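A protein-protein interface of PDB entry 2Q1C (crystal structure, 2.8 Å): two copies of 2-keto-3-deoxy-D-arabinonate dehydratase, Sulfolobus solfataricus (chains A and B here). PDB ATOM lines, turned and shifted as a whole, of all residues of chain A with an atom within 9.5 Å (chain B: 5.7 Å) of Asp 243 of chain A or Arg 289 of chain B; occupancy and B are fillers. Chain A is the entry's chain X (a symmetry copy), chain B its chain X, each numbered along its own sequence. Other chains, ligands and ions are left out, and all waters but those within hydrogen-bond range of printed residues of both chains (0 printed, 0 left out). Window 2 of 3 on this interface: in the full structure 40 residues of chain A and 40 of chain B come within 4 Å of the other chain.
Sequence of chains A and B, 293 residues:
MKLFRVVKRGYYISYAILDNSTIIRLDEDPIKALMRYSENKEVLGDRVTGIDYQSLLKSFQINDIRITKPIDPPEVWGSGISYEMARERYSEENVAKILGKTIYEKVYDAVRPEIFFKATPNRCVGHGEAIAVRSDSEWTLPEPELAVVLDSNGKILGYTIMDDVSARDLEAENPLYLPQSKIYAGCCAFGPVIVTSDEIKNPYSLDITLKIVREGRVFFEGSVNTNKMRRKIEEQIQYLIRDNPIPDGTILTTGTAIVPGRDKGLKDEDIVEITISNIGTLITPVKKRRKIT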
ATOM      1  N   TRP A  77       0.043   7.252  14.296  1.00  0.00           N
ATOM      2  CA  TRP A  77       0.981   8.369  14.236  1.00  0.00           C
ATOM      3  C   TRP A  77       1.446   8.763  15.631  1.00  0.00           C
ATOM      4  O   TRP A  77       0.738   8.546  16.618  1.00  0.00           O
ATOM      5  CB  TRP A  77       0.349   9.575  13.538  1.00  0.00           C
ATOM      6  CG  TRP A  77       0.153   9.408  12.060  1.00  0.00           C
ATOM      7  CD1 TRP A  77      -0.823   8.682  11.439  1.00  0.00           C
ATOM      8  CD2 TRP A  77       0.938   9.998  11.015  1.00  0.00           C
ATOM      9  NE1 TRP A  77      -0.690   8.775  10.077  1.00  0.00           N
ATOM     10  CE2 TRP A  77       0.382   9.578   9.788  1.00  0.00           C
ATOM     11  CE3 TRP A  77       2.058  10.841  10.998  1.00  0.00           C
ATOM     12  CZ2 TRP A  77       0.909   9.968   8.552  1.00  0.00           C
ATOM     13  CZ3 TRP A  77       2.582  11.230   9.767  1.00  0.00           C
ATOM     14  CH2 TRP A  77       2.006  10.791   8.563  1.00  0.00           C
ATOM     15  N   ARG A 112       5.866  24.757  15.244  1.00  0.00           N
ATOM     16  CA  ARG A 112       5.549  23.465  14.651  1.00  0.00           C
ATOM     17  C   ARG A 112       6.062  22.334  15.546  1.00  0.00           C
ATOM     18  O   ARG A 112       7.262  22.259  15.815  1.00  0.00           O
ATOM     19  CB  ARG A 112       6.178  23.371  13.258  1.00  0.00           C
ATOM     20  CG  ARG A 112       5.876  22.087  12.506  1.00  0.00           C
ATOM     21  CD  ARG A 112       6.674  21.996  11.207  1.00  0.00           C
ATOM     22  NE  ARG A 112       6.316  23.045  10.254  1.00  0.00           N
ATOM     23  CZ  ARG A 112       5.260  23.006   9.445  1.00  0.00           C
ATOM     24  NH1 ARG A 112       5.026  24.016   8.621  1.00  0.00           N
ATOM     25  NH2 ARG A 112       4.432  21.969   9.458  1.00  0.00           N
ATOM     26  N   ILE A 237      -3.142  17.348  16.701  1.00  0.00           N
ATOM     27  CA  ILE A 237      -4.104  16.898  15.690  1.00  0.00           C
ATOM     28  C   ILE A 237      -4.125  17.845  14.488  1.00  0.00           C
ATOM     29  O   ILE A 237      -4.176  17.397  13.339  1.00  0.00           O
ATOM     30  CB  ILE A 237      -5.533  16.759  16.279  1.00  0.00           C
ATOM     31  CG1 ILE A 237      -5.553  15.702  17.390  1.00  0.00           C
ATOM     32  CG2 ILE A 237      -6.541  16.406  15.186  1.00  0.00           C
ATOM     33  CD1 ILE A 237      -6.791  15.734  18.270  1.00  0.00           C
ATOM     34  N   GLN A 238      -4.073  19.147  14.767  1.00  0.00           N
ATOM     35  CA  GLN A 238      -4.085  20.182  13.737  1.00  0.00           C
ATOM     36  C   GLN A 238      -2.946  20.001  12.736  1.00  0.00           C
ATOM     37  O   GLN A 238      -3.160  20.074  11.526  1.00  0.00           O
ATOM     38  CB  GLN A 238      -4.005  21.567  14.383  1.00  0.00           C
ATOM     39  CG  GLN A 238      -4.283  22.727  13.435  1.00  0.00           C
ATOM     40  CD  GLN A 238      -3.716  24.050  13.933  1.00  0.00           C
ATOM     41  OE1 GLN A 238      -3.049  24.768  13.188  1.00  0.00           O
ATOM     42  NE2 GLN A 238      -3.977  24.376  15.198  1.00  0.00           N
ATOM     43  N   TYR A 239      -1.742  19.755  13.249  1.00  0.00           N
ATOM     44  CA  TYR A 239      -0.566  19.567  12.403  1.00  0.00           C
ATOM     45  C   TYR A 239      -0.513  18.186  11.749  1.00  0.00           C
ATOM     46  O   TYR A 239       0.133  18.009  10.713  1.00  0.00           O
ATOM     47  CB  TYR A 239       0.720  19.853  13.187  1.00  0.00           C
ATOM     48  CG  TYR A 239       1.053  21.327  13.261  1.00  0.00           C
ATOM     49  CD1 TYR A 239       0.479  22.145  14.236  1.00  0.00           C
ATOM     50  CD2 TYR A 239       1.928  21.907  12.344  1.00  0.00           C
ATOM     51  CE1 TYR A 239       0.777  23.503  14.302  1.00  0.00           C
ATOM     52  CE2 TYR A 239       2.230  23.264  12.400  1.00  0.00           C
ATOM     53  CZ  TYR A 239       1.653  24.055  13.381  1.00  0.00           C
ATOM     54  OH  TYR A 239       1.951  25.396  13.439  1.00  0.00           O
ATOM     55  N   LEU A 240      -1.197  17.217  12.352  1.00  0.00           N
ATOM     56  CA  LEU A 240      -1.289  15.873  11.788  1.00  0.00           C
ATOM     57  C   LEU A 240      -2.098  15.870  10.493  1.00  0.00           C
ATOM     58  O   LEU A 240      -1.646  15.338   9.479  1.00  0.00           O
ATOM     59  CB  LEU A 240      -1.896  14.894  12.805  1.00  0.00           C
ATOM     60  CG  LEU A 240      -2.230  13.470  12.342  1.00  0.00           C
ATOM     61  CD1 LEU A 240      -0.985  12.716  11.917  1.00  0.00           C
ATOM     62  CD2 LEU A 240      -2.971  12.706  13.422  1.00  0.00           C
ATOM     63  N   ILE A 241      -3.283  16.479  10.535  1.00  0.00           N
ATOM     64  CA  ILE A 241      -4.228  16.429   9.408  1.00  0.00           C
ATOM     65  C   ILE A 241      -3.959  17.439   8.288  1.00  0.00           C
ATOM     66  O   ILE A 241      -4.520  17.308   7.199  1.00  0.00           O
ATOM     67  CB  ILE A 241      -5.715  16.522   9.876  1.00  0.00           C
ATOM     68  CG1 ILE A 241      -5.993  17.853  10.590  1.00  0.00           C
ATOM     69  CG2 ILE A 241      -6.073  15.327  10.754  1.00  0.00           C
ATOM     70  CD1 ILE A 241      -7.463  18.108  10.905  1.00  0.00           C
ATOM     71  N   ARG A 242      -3.101  18.427   8.551  1.00  0.00           N
ATOM     72  CA  ARG A 242      -2.790  19.481   7.577  1.00  0.00           C
ATOM     73  C   ARG A 242      -2.250  18.917   6.263  1.00  0.00           C
ATOM     74  O   ARG A 242      -1.162  18.329   6.235  1.00  0.00           O
ATOM     75  CB  ARG A 242      -1.800  20.492   8.167  1.00  0.00           C
ATOM     76  CG  ARG A 242      -1.309  21.531   7.161  1.00  0.00           C
ATOM     77  CD  ARG A 242      -0.321  22.501   7.776  1.00  0.00           C
ATOM     78  NE  ARG A 242      -0.955  23.377   8.760  1.00  0.00           N
ATOM     79  CZ  ARG A 242      -0.329  24.340   9.430  1.00  0.00           C
ATOM     80  NH1 ARG A 242       0.963  24.571   9.234  1.00  0.00           N
ATOM     81  NH2 ARG A 242      -1.003  25.077  10.302  1.00  0.00           N
ATOM     82  N   ASP A 243      -3.020  19.104   5.186  1.00  0.00           N
ATOM     83  CA  ASP A 243      -2.697  18.578   3.846  1.00  0.00           C
ATOM     84  C   ASP A 243      -2.451  17.066   3.841  1.00  0.00           C
ATOM     85  O   ASP A 243      -1.894  16.510   2.890  1.00  0.00           O
ATOM     86  CB  ASP A 243      -1.497  19.318   3.239  1.00  0.00           C
ATOM     87  CG  ASP A 243      -1.784  20.779   2.969  1.00  0.00           C
ATOM     88  OD1 ASP A 243      -2.967  21.145   2.807  1.00  0.00           O
ATOM     89  OD2 ASP A 243      -0.817  21.566   2.910  1.00  0.00           O
ATOM     90  N   ASN A 244      -2.888  16.413   4.913  1.00  0.00           N
ATOM     91  CA  ASN A 244      -2.614  15.009   5.142  1.00  0.00           C
ATOM     92  C   ASN A 244      -3.875  14.293   5.616  1.00  0.00           C
ATOM     93  O   ASN A 244      -4.196  14.320   6.804  1.00  0.00           O
ATOM     94  CB  ASN A 244      -1.487  14.865   6.165  1.00  0.00           C
ATOM     95  CG  ASN A 244      -0.982  13.447   6.286  1.00  0.00           C
ATOM     96  OD1 ASN A 244      -0.894  12.715   5.300  1.00  0.00           O
ATOM     97  ND2 ASN A 244      -0.637  13.051   7.506  1.00  0.00           N
ATOM     98  N   PRO A 245      -4.608  13.662   4.681  1.00  0.00           N
ATOM     99  CA  PRO A 245      -5.832  12.953   5.042  1.00  0.00           C
ATOM    100  C   PRO A 245      -5.535  11.687   5.837  1.00  0.00           C
ATOM    101  O   PRO A 245      -4.664  10.900   5.457  1.00  0.00           O
ATOM    102  CB  PRO A 245      -6.454  12.606   3.685  1.00  0.00           C
ATOM    103  CG  PRO A 245      -5.304  12.546   2.745  1.00  0.00           C
ATOM    104  CD  PRO A 245      -4.325  13.576   3.235  1.00  0.00           C
ATOM    105  N   ILE A 246      -6.251  11.517   6.942  1.00  0.00           N
ATOM    106  CA  ILE A 246      -6.146  10.314   7.762  1.00  0.00           C
ATOM    107  C   ILE A 246      -7.460   9.532   7.715  1.00  0.00           C
ATOM    108  O   ILE A 246      -8.534  10.131   7.709  1.00  0.00           O
ATOM    109  CB  ILE A 246      -5.745  10.632   9.230  1.00  0.00           C
ATOM    110  CG1 ILE A 246      -6.705  11.656   9.857  1.00  0.00           C
ATOM    111  CG2 ILE A 246      -4.292  11.117   9.290  1.00  0.00           C
ATOM    112  CD1 ILE A 246      -6.683  11.695  11.376  1.00  0.00           C
ATOM    113  N   ALA B 132       1.619  17.418  -5.283  1.00  0.00           N
ATOM    114  CA  ALA B 132       1.244  18.569  -4.459  1.00  0.00           C
ATOM    115  C   ALA B 132       2.393  19.244  -3.710  1.00  0.00           C
ATOM    116  O   ALA B 132       3.390  18.612  -3.359  1.00  0.00           O
ATOM    117  CB  ALA B 132       0.129  18.187  -3.488  1.00  0.00           C
ATOM    118  N   VAL B 133       2.229  20.546  -3.488  1.00  0.00           N
ATOM    119  CA  VAL B 133       3.100  21.333  -2.628  1.00  0.00           C
ATOM    120  C   VAL B 133       2.283  21.706  -1.396  1.00  0.00           C
ATOM    121  O   VAL B 133       1.215  22.310  -1.523  1.00  0.00           O
ATOM    122  CB  VAL B 133       3.588  22.627  -3.333  1.00  0.00           C
ATOM    123  CG1 VAL B 133       4.443  23.473  -2.394  1.00  0.00           C
ATOM    124  CG2 VAL B 133       4.363  22.297  -4.602  1.00  0.00           C
ATOM    125  N   ARG B 134       2.780  21.341  -0.216  1.00  0.00           N
ATOM    126  CA  ARG B 134       2.111  21.657   1.054  1.00  0.00           C
ATOM    127  C   ARG B 134       1.759  23.139   1.159  1.00  0.00           C
ATOM    128  O   ARG B 134       2.504  23.994   0.675  1.00  0.00           O
ATOM    129  CB  ARG B 134       2.999  21.270   2.238  1.00  0.00           C
ATOM    130  CG  ARG B 134       3.172  19.774   2.462  1.00  0.00           C
ATOM    131  CD  ARG B 134       3.979  19.520   3.729  1.00  0.00           C
ATOM    132  NE  ARG B 134       3.364  20.159   4.892  1.00  0.00           N
ATOM    133  CZ  ARG B 134       2.700  19.519   5.849  1.00  0.00           C
ATOM    134  NH1 ARG B 134       2.569  18.197   5.812  1.00  0.00           N
ATOM    135  NH2 ARG B 134       2.173  20.205   6.855  1.00  0.00           N
ATOM    136  N   SER B 135       0.633  23.439   1.801  1.00  0.00           N
ATOM    137  CA  SER B 135       0.177  24.825   1.952  1.00  0.00           C
ATOM    138  C   SER B 135       1.158  25.698   2.740  1.00  0.00           C
ATOM    139  O   SER B 135       1.205  26.915   2.545  1.00  0.00           O
ATOM    140  CB  SER B 135      -1.212  24.879   2.598  1.00  0.00           C
ATOM    141  OG  SER B 135      -1.153  24.598   3.985  1.00  0.00           O
ATOM    142  N   ASP B 136       1.940  25.069   3.614  1.00  0.00           N
ATOM    143  CA  ASP B 136       2.874  25.780   4.485  1.00  0.00           C
ATOM    144  C   ASP B 136       4.342  25.595   4.086  1.00  0.00           C
ATOM    145  O   ASP B 136       5.241  25.748   4.919  1.00  0.00           O
ATOM    146  CB  ASP B 136       2.654  25.369   5.948  1.00  0.00           C
ATOM    147  CG  ASP B 136       2.824  23.864   6.181  1.00  0.00           C
ATOM    148  OD1 ASP B 136       3.060  23.105   5.211  1.00  0.00           O
ATOM    149  OD2 ASP B 136       2.719  23.439   7.349  1.00  0.00           O
ATOM    150  N   TYR B 184       2.438  13.332   2.817  1.00  0.00           N
ATOM    151  CA  TYR B 184       1.194  14.101   2.683  1.00  0.00           C
ATOM    152  C   TYR B 184       0.431  13.699   1.419  1.00  0.00           C
ATOM    153  O   TYR B 184       0.898  12.858   0.651  1.00  0.00           O
ATOM    154  CB  TYR B 184       1.471  15.615   2.700  1.00  0.00           C
ATOM    155  CG  TYR B 184       2.466  16.089   1.659  1.00  0.00           C
ATOM    156  CD1 TYR B 184       2.037  16.523   0.406  1.00  0.00           C
ATOM    157  CD2 TYR B 184       3.833  16.113   1.931  1.00  0.00           C
ATOM    158  CE1 TYR B 184       2.941  16.960  -0.552  1.00  0.00           C
ATOM    159  CE2 TYR B 184       4.749  16.548   0.976  1.00  0.00           C
ATOM    160  CZ  TYR B 184       4.294  16.970  -0.263  1.00  0.00           C
ATOM    161  OH  TYR B 184       5.187  17.406  -1.214  1.00  0.00           O
ATOM    162  N   ALA B 185      -0.743  14.293   1.211  1.00  0.00           N
ATOM    163  CA  ALA B 185      -1.549  14.019   0.018  1.00  0.00           C
ATOM    164  C   ALA B 185      -0.838  14.499  -1.245  1.00  0.00           C
ATOM    165  O   ALA B 185      -0.514  15.678  -1.374  1.00  0.00           O
ATOM    166  CB  ALA B 185      -2.922  14.665   0.137  1.00  0.00           C
ATOM    167  N   GLY B 186      -0.592  13.572  -2.166  1.00  0.00           N
ATOM    168  CA  GLY B 186       0.100  13.880  -3.414  1.00  0.00           C
ATOM    169  C   GLY B 186       1.596  14.089  -3.243  1.00  0.00           C
ATOM    170  O   GLY B 186       2.217  14.829  -4.011  1.00  0.00           O
ATOM    171  N   LYS B 287       0.192  21.034  -8.165  1.00  0.00           N
ATOM    172  CA  LYS B 287      -0.950  21.730  -7.586  1.00  0.00           C
ATOM    173  C   LYS B 287      -0.618  22.227  -6.176  1.00  0.00           C
ATOM    174  O   LYS B 287      -0.383  21.429  -5.265  1.00  0.00           O
ATOM    175  CB  LYS B 287      -2.184  20.809  -7.583  1.00  0.00           C
ATOM    176  CG  LYS B 287      -3.367  21.288  -6.737  1.00  0.00           C
ATOM    177  CD  LYS B 287      -4.062  22.502  -7.347  1.00  0.00           C
ATOM    178  CE  LYS B 287      -5.041  23.129  -6.365  1.00  0.00           C
ATOM    179  NZ  LYS B 287      -5.623  24.391  -6.900  1.00  0.00           N
ATOM    180  N   LYS B 288      -0.598  23.548  -6.012  1.00  0.00           N
ATOM    181  CA  LYS B 288      -0.304  24.176  -4.724  1.00  0.00           C
ATOM    182  C   LYS B 288      -1.509  24.092  -3.788  1.00  0.00           C
ATOM    183  O   LYS B 288      -2.619  24.473  -4.163  1.00  0.00           O
ATOM    184  CB  LYS B 288       0.124  25.636  -4.932  1.00  0.00           C
ATOM    185  CG  LYS B 288       0.253  26.470  -3.658  1.00  0.00           C
ATOM    186  CD  LYS B 288       1.556  26.204  -2.917  1.00  0.00           C
ATOM    187  CE  LYS B 288       1.587  26.954  -1.594  1.00  0.00           C
ATOM    188  NZ  LYS B 288       2.910  26.850  -0.923  1.00  0.00           N
ATOM    189  N   ARG B 289      -1.284  23.593  -2.575  1.00  0.00           N
ATOM    190  CA  ARG B 289      -2.355  23.460  -1.587  1.00  0.00           C
ATOM    191  C   ARG B 289      -2.754  24.804  -0.985  1.00  0.00           C
ATOM    192  O   ARG B 289      -1.903  25.644  -0.684  1.00  0.00           O
ATOM    193  CB  ARG B 289      -1.967  22.487  -0.468  1.00  0.00           C
ATOM    194  CG  ARG B 289      -1.849  21.025  -0.888  1.00  0.00           C
ATOM    195  CD  ARG B 289      -3.196  20.405  -1.239  1.00  0.00           C
ATOM    196  NE  ARG B 289      -3.065  18.975  -1.515  1.00  0.00           N
ATOM    197  CZ  ARG B 289      -3.797  18.305  -2.403  1.00  0.00           C
ATOM    198  NH1 ARG B 289      -3.598  17.004  -2.577  1.00  0.00           N
ATOM    199  NH2 ARG B 289      -4.721  18.929  -3.126  1.00  0.00           N
ATOM    200  N   ARG B 290      -4.062  24.987  -0.820  1.00  0.00           N
ATOM    201  CA  ARG B 290      -4.626  26.178  -0.195  1.00  0.00           C
ATOM    202  C   ARG B 290      -4.688  25.973   1.321  1.00  0.00           C
ATOM    203  O   ARG B 290      -4.962  24.863   1.791  1.00  0.00           O
ATOM    204  CB  ARG B 290      -6.024  26.449  -0.767  1.00  0.00           C
ATOM    205  CG  ARG B 290      -6.661  27.763  -0.337  1.00  0.00           C
ATOM    206  CD  ARG B 290      -8.143  27.793  -0.691  1.00  0.00           C
ATOM    207  NE  ARG B 290      -8.792  29.018  -0.221  1.00  0.00           N
ATOM    208  CZ  ARG B 290      -9.027  30.090  -0.977  1.00  0.00           C
ATOM    209  NH1 ARG B 290      -8.677  30.103  -2.260  1.00  0.00           N
ATOM    210  NH2 ARG B 290      -9.621  31.155  -0.449  1.00  0.00           N
ATOM    211  N   LYS B 291      -4.429  27.041   2.076  1.00  0.00           N
ATOM    212  CA  LYS B 291      -4.389  26.983   3.543  1.00  0.00           C
ATOM    213  C   LYS B 291      -5.770  26.787   4.165  1.00  0.00           C
ATOM    214  O   LYS B 291      -6.729  27.470   3.807  1.00  0.00           O
ATOM    215  CB  LYS B 291      -3.717  28.236   4.118  1.00  0.00           C
ATOM    216  CG  LYS B 291      -2.236  28.353   3.779  1.00  0.00           C
ATOM    217  CD  LYS B 291      -1.611  29.599   4.383  1.00  0.00           C
ATOM    218  CE  LYS B 291      -0.121  29.663   4.073  1.00  0.00           C
ATOM    219  NZ  LYS B 291       0.522  30.879   4.650  1.00  0.00           N
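OD2 of Asp 136 of chain B lies within salt-bridge range of NH1 of Arg 242 of chain A (2.8 Å).
The side-chain carboxylate (OD2) of Asp 136 of chain B lies within salt-bridge range of the guanidinium group (NH1) of Arg 112 of chain A, 2.7 Å away.
N of Ala 185 of chain B lies within hydrogen-bond range of O of Asp 243 of chain A, at 3.0 Å.
OD2 of Asp 243 of chain A sits at hydrogen-bond distance from N of Ser 135 of chain B (2.6 Å).
O of Leu 240 of chain A is in hydrogen-bond range of ND2 of Asn 244 of chain A, 3.2 Å away.
The side-chain amino group (NZ) of Lys 288 of chain B sits at hydrogen-bond distance from the backbone carbonyl oxygen (O) of Arg 134 of chain B.
The backbone carbonyl oxygen (O) of Ala 132 of chain B lies within hydrogen-bond range of the side-chain hydroxyl (OH) of Tyr 184 of chain B, 3.0 Å away.
The side-chain carboxylate (OD1) of Asp 136 of chain B lies within salt-bridge range of the guanidinium group (NE) of Arg 134 of chain B (3.0 Å).
The backbone NH (N) of Arg 289 of chain B is in hydrogen-bond range of the backbone carbonyl oxygen (O) of Val 133 of chain B.
Arg 112 of chain A touches Arg 134 of chain B.
Arg 242 of chain A touches Arg 134 of chain B.
Asp 243 of chain A touches Arg 134 of chain B.
Tyr 184 of chain B touches Asp 243 of chain A (CB to O, 3.5 Å).
OD1 of Asp 243 of chain A touches CB of Arg 289 of chain B, 3.7 Å away.
Tyr 184 of chain B touches Asn 244 of chain A (CA to OD1, 3.6 Å).
Ala 185 of chain B touches Pro 245 of chain A (CB to CD, 3.6 Å).
Printed residues of chain B within 4 Å of Arg 112 of chain A: Arg 134 (3.9 Å) and Asp 136 (2.7 Å).
Of the printed residues of chain B, Arg 242 of chain A touches Arg 134 (3.5 Å) and Asp 136 (2.8 Å).
Asp 243 of chain A touches five residues of chain B.
Of chain A, only Arg 112, Arg 242 and Asp 243 come within 4 Å of Arg 134 of chain B.
Printed residues of chain A within 4 Å of Asp 136 of chain B: Arg 112 and Arg 242.
Of chain A, only Asp 243 comes within 4 Å of Arg 289 of chain B.
The nearest residue of chain B that does not touch Asp 243 of chain A is Arg 290 of chain B (4.3 Å).
The nearest residue of chain A that does not touch Arg 289 of chain B is Pro 245 of chain A (6.8 Å).
Printed residues of chain A that touch a printed residue of chain B: Arg 112, Arg 242, Asp 243, Asn 244 and Pro 245.
Hydrophobic or aromatic side chains of chain A that line the printed part of chain B: Pro 245.
Of the 13 printed residues of chain B, 6 touch a printed residue of chain A.
Hydrophobic or aromatic side chains of chain B that line the printed part of chain A: Tyr 184 and Ala 185.
Among the printed residues, 11 pairs touch across the chains.
Among the printed residues, Asp or Glu carboxylates within 4 Å of a Lys or Arg side-chain nitrogen of the other chain: Arg 112 of chain A with Asp 136 of chain B (2.7 Å) and Arg 242 of chain A with Asp 136 of chain B (2.8 Å).
No position is printed for both chains.
Of the 11 pairs that touch across the chains among the printed residues, none has its exchanged pair printed and touching as well.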
